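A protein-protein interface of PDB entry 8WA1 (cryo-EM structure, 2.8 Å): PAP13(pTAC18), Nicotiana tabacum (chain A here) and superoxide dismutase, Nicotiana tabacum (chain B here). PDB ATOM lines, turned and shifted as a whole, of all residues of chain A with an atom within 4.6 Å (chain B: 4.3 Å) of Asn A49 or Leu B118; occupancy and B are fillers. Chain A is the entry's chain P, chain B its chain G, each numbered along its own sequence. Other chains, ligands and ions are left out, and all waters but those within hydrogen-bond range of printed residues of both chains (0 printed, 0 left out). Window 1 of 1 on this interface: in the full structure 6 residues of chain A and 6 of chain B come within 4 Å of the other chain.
Among the printed residues, pairs that only touch across the chains: Arg A51 with Pro B119 (3.3 Å), Asn A49 with Leu B118 (3.4 Å) and Asn A49 with Asn B113 (3.6 Å).
The backbone carbonyl oxygen of Thr B111 lies within hydrogen-bond range of the backbone NH of Leu B118, 2.6 Å away.
Of chain B, only Asn B113 and Leu B118 come within 4 Å of Asn A49.
Of the printed residues of chain B, Arg A51 touches Pro B119.
Thr B111 touches none of the printed residues of chain A.
Of the printed residues of chain A, Asn B113 touches Asn A49.
Of the printed residues of chain A, Pro B119 touches Arg A51 (3.3 Å).
The nearest printed residue of chain A that does not touch Pro B119 is Asn A49 (6.7 Å).
Hydrophobic or aromatic side chains of chain B that line the printed part of chain A: Leu B118 and Pro B119.
Among the printed residues, no Asp or Glu carboxylate lies within 4 Å of a Lys or Arg side-chain nitrogen of the other chain.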
ATOM      1  N   GLU A  45      16.584   4.218 -10.511  1.00  0.00           N
ATOM      2  CA  GLU A  45      17.680   3.587 -11.240  1.00  0.00           C
ATOM      3  C   GLU A  45      18.452   2.626 -10.343  1.00  0.00           C
ATOM      4  O   GLU A  45      18.943   1.590 -10.808  1.00  0.00           O
ATOM      5  CB  GLU A  45      18.614   4.651 -11.819  1.00  0.00           C
ATOM      6  CG  GLU A  45      18.428   6.046 -11.240  1.00  0.00           C
ATOM      7  CD  GLU A  45      17.339   6.833 -11.946  1.00  0.00           C
ATOM      8  OE1 GLU A  45      16.773   6.315 -12.931  1.00  0.00           O
ATOM      9  OE2 GLU A  45      17.050   7.970 -11.517  1.00  0.00           O
ATOM     10  N   GLU A  46      18.566   2.952  -9.055  1.00  0.00           N
ATOM     11  CA  GLU A  46      19.258   2.063  -8.128  1.00  0.00           C
ATOM     12  C   GLU A  46      18.419   0.831  -7.810  1.00  0.00           C
ATOM     13  O   GLU A  46      18.956  -0.276  -7.677  1.00  0.00           O
ATOM     14  CB  GLU A  46      19.614   2.817  -6.847  1.00  0.00           C
ATOM     15  CG  GLU A  46      20.541   2.055  -5.916  1.00  0.00           C
ATOM     16  CD  GLU A  46      21.928   1.864  -6.501  1.00  0.00           C
ATOM     17  OE1 GLU A  46      22.315   2.647  -7.394  1.00  0.00           O
ATOM     18  OE2 GLU A  46      22.633   0.929  -6.067  1.00  0.00           O
ATOM     19  N   LEU A  47      17.099   1.001  -7.681  1.00  0.00           N
ATOM     20  CA  LEU A  47      16.235  -0.130  -7.349  1.00  0.00           C
ATOM     21  C   LEU A  47      16.220  -1.167  -8.465  1.00  0.00           C
ATOM     22  O   LEU A  47      16.380  -2.366  -8.211  1.00  0.00           O
ATOM     23  CB  LEU A  47      14.813   0.353  -7.058  1.00  0.00           C
ATOM     24  CG  LEU A  47      14.495   0.906  -5.665  1.00  0.00           C
ATOM     25  CD1 LEU A  47      14.962   2.344  -5.514  1.00  0.00           C
ATOM     26  CD2 LEU A  47      13.006   0.792  -5.374  1.00  0.00           C
ATOM     27  N   TYR A  48      16.037  -0.725  -9.708  1.00  0.00           N
ATOM     28  CA  TYR A  48      15.954  -1.623 -10.851  1.00  0.00           C
ATOM     29  C   TYR A  48      17.306  -1.856 -11.512  1.00  0.00           C
ATOM     30  O   TYR A  48      17.356  -2.409 -12.615  1.00  0.00           O
ATOM     31  CB  TYR A  48      14.952  -1.084 -11.874  1.00  0.00           C
ATOM     32  CG  TYR A  48      13.508  -1.242 -11.453  1.00  0.00           C
ATOM     33  CD1 TYR A  48      12.900  -0.313 -10.621  1.00  0.00           C
ATOM     34  CD2 TYR A  48      12.754  -2.327 -11.886  1.00  0.00           C
ATOM     35  CE1 TYR A  48      11.582  -0.457 -10.233  1.00  0.00           C
ATOM     36  CE2 TYR A  48      11.435  -2.477 -11.504  1.00  0.00           C
ATOM     37  CZ  TYR A  48      10.855  -1.541 -10.677  1.00  0.00           C
ATOM     38  OH  TYR A  48       9.542  -1.687 -10.295  1.00  0.00           O
ATOM     39  N   ASN A  49      18.396  -1.444 -10.858  1.00  0.00           N
ATOM     40  CA  ASN A  49      19.758  -1.674 -11.345  1.00  0.00           C
ATOM     41  C   ASN A  49      19.959  -1.078 -12.737  1.00  0.00           C
ATOM     42  O   ASN A  49      20.676  -1.628 -13.574  1.00  0.00           O
ATOM     43  CB  ASN A  49      20.104  -3.166 -11.331  1.00  0.00           C
ATOM     44  CG  ASN A  49      21.598  -3.420 -11.362  1.00  0.00           C
ATOM     45  OD1 ASN A  49      22.164  -3.743 -12.406  1.00  0.00           O
ATOM     46  ND2 ASN A  49      22.248  -3.272 -10.213  1.00  0.00           N
ATOM     47  N   VAL A  50      19.319   0.060 -12.985  1.00  0.00           N
ATOM     48  CA  VAL A  50      19.421   0.764 -14.257  1.00  0.00           C
ATOM     49  C   VAL A  50      20.614   1.706 -14.182  1.00  0.00           C
ATOM     50  O   VAL A  50      20.556   2.743 -13.509  1.00  0.00           O
ATOM     51  CB  VAL A  50      18.130   1.529 -14.582  1.00  0.00           C
ATOM     52  CG1 VAL A  50      18.251   2.222 -15.928  1.00  0.00           C
ATOM     53  CG2 VAL A  50      16.937   0.585 -14.568  1.00  0.00           C
ATOM     54  N   ARG A  51      21.695   1.350 -14.867  1.00  0.00           N
ATOM     55  CA  ARG A  51      22.925   2.129 -14.866  1.00  0.00           C
ATOM     56  C   ARG A  51      22.889   3.127 -16.014  1.00  0.00           C
ATOM     57  O   ARG A  51      22.756   2.738 -17.179  1.00  0.00           O
ATOM     58  CB  ARG A  51      24.146   1.216 -14.984  1.00  0.00           C
ATOM     59  CG  ARG A  51      24.381   0.340 -13.764  1.00  0.00           C
ATOM     60  CD  ARG A  51      25.364  -0.781 -14.059  1.00  0.00           C
ATOM     61  NE  ARG A  51      24.789  -1.798 -14.936  1.00  0.00           N
ATOM     62  CZ  ARG A  51      25.450  -2.864 -15.375  1.00  0.00           C
ATOM     63  NH1 ARG A  51      26.713  -3.054 -15.022  1.00  0.00           N
ATOM     64  NH2 ARG A  51      24.848  -3.740 -16.168  1.00  0.00           N
ATOM     65  N   PRO A 118      18.687  -3.412 -17.801  1.00  0.00           N
ATOM     66  CA  PRO A 118      19.029  -4.742 -17.286  1.00  0.00           C
ATOM     67  C   PRO A 118      18.184  -5.835 -17.924  1.00  0.00           C
ATOM     68  O   PRO A 118      17.191  -5.582 -18.610  1.00  0.00           O
ATOM     69  CB  PRO A 118      18.738  -4.631 -15.783  1.00  0.00           C
ATOM     70  CG  PRO A 118      18.592  -3.159 -15.510  1.00  0.00           C
ATOM     71  CD  PRO A 118      18.058  -2.571 -16.772  1.00  0.00           C
ATOM     72  N   VAL B 110      24.843  -8.986  -3.261  1.00  0.00           N
ATOM     73  CA  VAL B 110      24.199  -7.888  -3.972  1.00  0.00           C
ATOM     74  C   VAL B 110      24.698  -7.815  -5.409  1.00  0.00           C
ATOM     75  O   VAL B 110      23.914  -7.615  -6.344  1.00  0.00           O
ATOM     76  CB  VAL B 110      24.420  -6.562  -3.222  1.00  0.00           C
ATOM     77  CG1 VAL B 110      24.014  -5.383  -4.090  1.00  0.00           C
ATOM     78  CG2 VAL B 110      23.630  -6.555  -1.923  1.00  0.00           C
ATOM     79  N   THR B 111      26.007  -7.986  -5.614  1.00  0.00           N
ATOM     80  CA  THR B 111      26.557  -7.914  -6.964  1.00  0.00           C
ATOM     81  C   THR B 111      26.117  -9.094  -7.820  1.00  0.00           C
ATOM     82  O   THR B 111      26.101  -8.989  -9.050  1.00  0.00           O
ATOM     83  CB  THR B 111      28.082  -7.839  -6.911  1.00  0.00           C
ATOM     84  OG1 THR B 111      28.585  -8.879  -6.064  1.00  0.00           O
ATOM     85  CG2 THR B 111      28.532  -6.490  -6.376  1.00  0.00           C
ATOM     86  N   ASN B 113      23.079 -10.185  -7.931  1.00  0.00           N
ATOM     87  CA  ASN B 113      21.863  -9.588  -8.486  1.00  0.00           C
ATOM     88  C   ASN B 113      20.931 -10.646  -9.079  1.00  0.00           C
ATOM     89  O   ASN B 113      20.289 -10.436 -10.111  1.00  0.00           O
ATOM     90  CB  ASN B 113      22.211  -8.513  -9.522  1.00  0.00           C
ATOM     91  CG  ASN B 113      21.040  -7.603  -9.834  1.00  0.00           C
ATOM     92  OD1 ASN B 113      20.112  -7.471  -9.038  1.00  0.00           O
ATOM     93  ND2 ASN B 113      21.078  -6.973 -11.003  1.00  0.00           N
ATOM     94  N   ASN B 116      22.139 -12.069 -12.628  1.00  0.00           N
ATOM     95  CA  ASN B 116      22.811 -11.110 -13.504  1.00  0.00           C
ATOM     96  C   ASN B 116      23.974 -10.491 -12.745  1.00  0.00           C
ATOM     97  O   ASN B 116      23.798  -9.467 -12.060  1.00  0.00           O
ATOM     98  CB  ASN B 116      21.842 -10.030 -13.983  1.00  0.00           C
ATOM     99  CG  ASN B 116      22.246  -9.439 -15.319  1.00  0.00           C
ATOM    100  OD1 ASN B 116      21.433  -9.348 -16.237  1.00  0.00           O
ATOM    101  ND2 ASN B 116      23.506  -9.043 -15.437  1.00  0.00           N
ATOM    102  N   PRO B 117      25.174 -11.064 -12.832  1.00  0.00           N
ATOM    103  CA  PRO B 117      26.294 -10.550 -12.036  1.00  0.00           C
ATOM    104  C   PRO B 117      26.674  -9.134 -12.443  1.00  0.00           C
ATOM    105  O   PRO B 117      26.701  -8.791 -13.626  1.00  0.00           O
ATOM    106  CB  PRO B 117      27.425 -11.542 -12.333  1.00  0.00           C
ATOM    107  CG  PRO B 117      26.739 -12.770 -12.855  1.00  0.00           C
ATOM    108  CD  PRO B 117      25.540 -12.268 -13.594  1.00  0.00           C
ATOM    109  N   LEU B 118      26.968  -8.313 -11.442  1.00  0.00           N
ATOM    110  CA  LEU B 118      27.436  -6.955 -11.665  1.00  0.00           C
ATOM    111  C   LEU B 118      28.919  -6.977 -12.014  1.00  0.00           C
ATOM    112  O   LEU B 118      29.612  -7.969 -11.772  1.00  0.00           O
ATOM    113  CB  LEU B 118      27.162  -6.109 -10.422  1.00  0.00           C
ATOM    114  CG  LEU B 118      25.687  -5.867 -10.091  1.00  0.00           C
ATOM    115  CD1 LEU B 118      25.546  -4.917  -8.910  1.00  0.00           C
ATOM    116  CD2 LEU B 118      24.944  -5.333 -11.305  1.00  0.00           C
ATOM    117  N   PRO B 119      29.445  -5.894 -12.596  1.00  0.00           N
ATOM    118  CA  PRO B 119      30.874  -5.882 -12.952  1.00  0.00           C
ATOM    119  C   PRO B 119      31.808  -5.980 -11.757  1.00  0.00           C
ATOM    120  O   PRO B 119      33.010  -6.201 -11.951  1.00  0.00           O
ATOM    121  CB  PRO B 119      31.043  -4.546 -13.690  1.00  0.00           C
ATOM    122  CG  PRO B 119      29.891  -3.710 -13.240  1.00  0.00           C
ATOM    123  CD  PRO B 119      28.761  -4.670 -13.048  1.00  0.00           C
ATOM    124  N   GLU B 120      31.303  -5.824 -10.535  1.00  0.00           N
ATOM    125  CA  GLU B 120      32.113  -5.953  -9.331  1.00  0.00           C
ATOM    126  C   GLU B 120      31.940  -7.299  -8.639  1.00  0.00           C
ATOM    127  O   GLU B 120      32.614  -7.556  -7.637  1.00  0.00           O
ATOM    128  CB  GLU B 120      31.787  -4.818  -8.354  1.00  0.00           C
ATOM    129  CG  GLU B 120      32.190  -3.443  -8.863  1.00  0.00           C
ATOM    130  CD  GLU B 120      31.881  -2.329  -7.879  1.00  0.00           C
ATOM    131  OE1 GLU B 120      30.858  -1.638  -8.061  1.00  0.00           O
ATOM    132  OE2 GLU B 120      32.665  -2.144  -6.924  1.00  0.00           O
ATOM    133  N   PHE B 121      31.055  -8.162  -9.145  1.00  0.00           N
ATOM    134  CA  PHE B 121      30.877  -9.481  -8.544  1.00  0.00           C
ATOM    135  C   PHE B 121      32.124 -10.338  -8.712  1.00  0.00           C
ATOM    136  O   PHE B 121      32.533 -11.047  -7.782  1.00  0.00           O
ATOM    137  CB  PHE B 121      29.661 -10.172  -9.162  1.00  0.00           C
ATOM    138  CG  PHE B 121      29.514 -11.618  -8.773  1.00  0.00           C
ATOM    139  CD1 PHE B 121      29.131 -11.970  -7.490  1.00  0.00           C
ATOM    140  CD2 PHE B 121      29.743 -12.625  -9.699  1.00  0.00           C
ATOM    141  CE1 PHE B 121      28.991 -13.300  -7.133  1.00  0.00           C
ATOM    142  CE2 PHE B 121      29.604 -13.955  -9.347  1.00  0.00           C
ATOM    143  CZ  PHE B 121      29.228 -14.293  -8.062  1.00  0.00           C
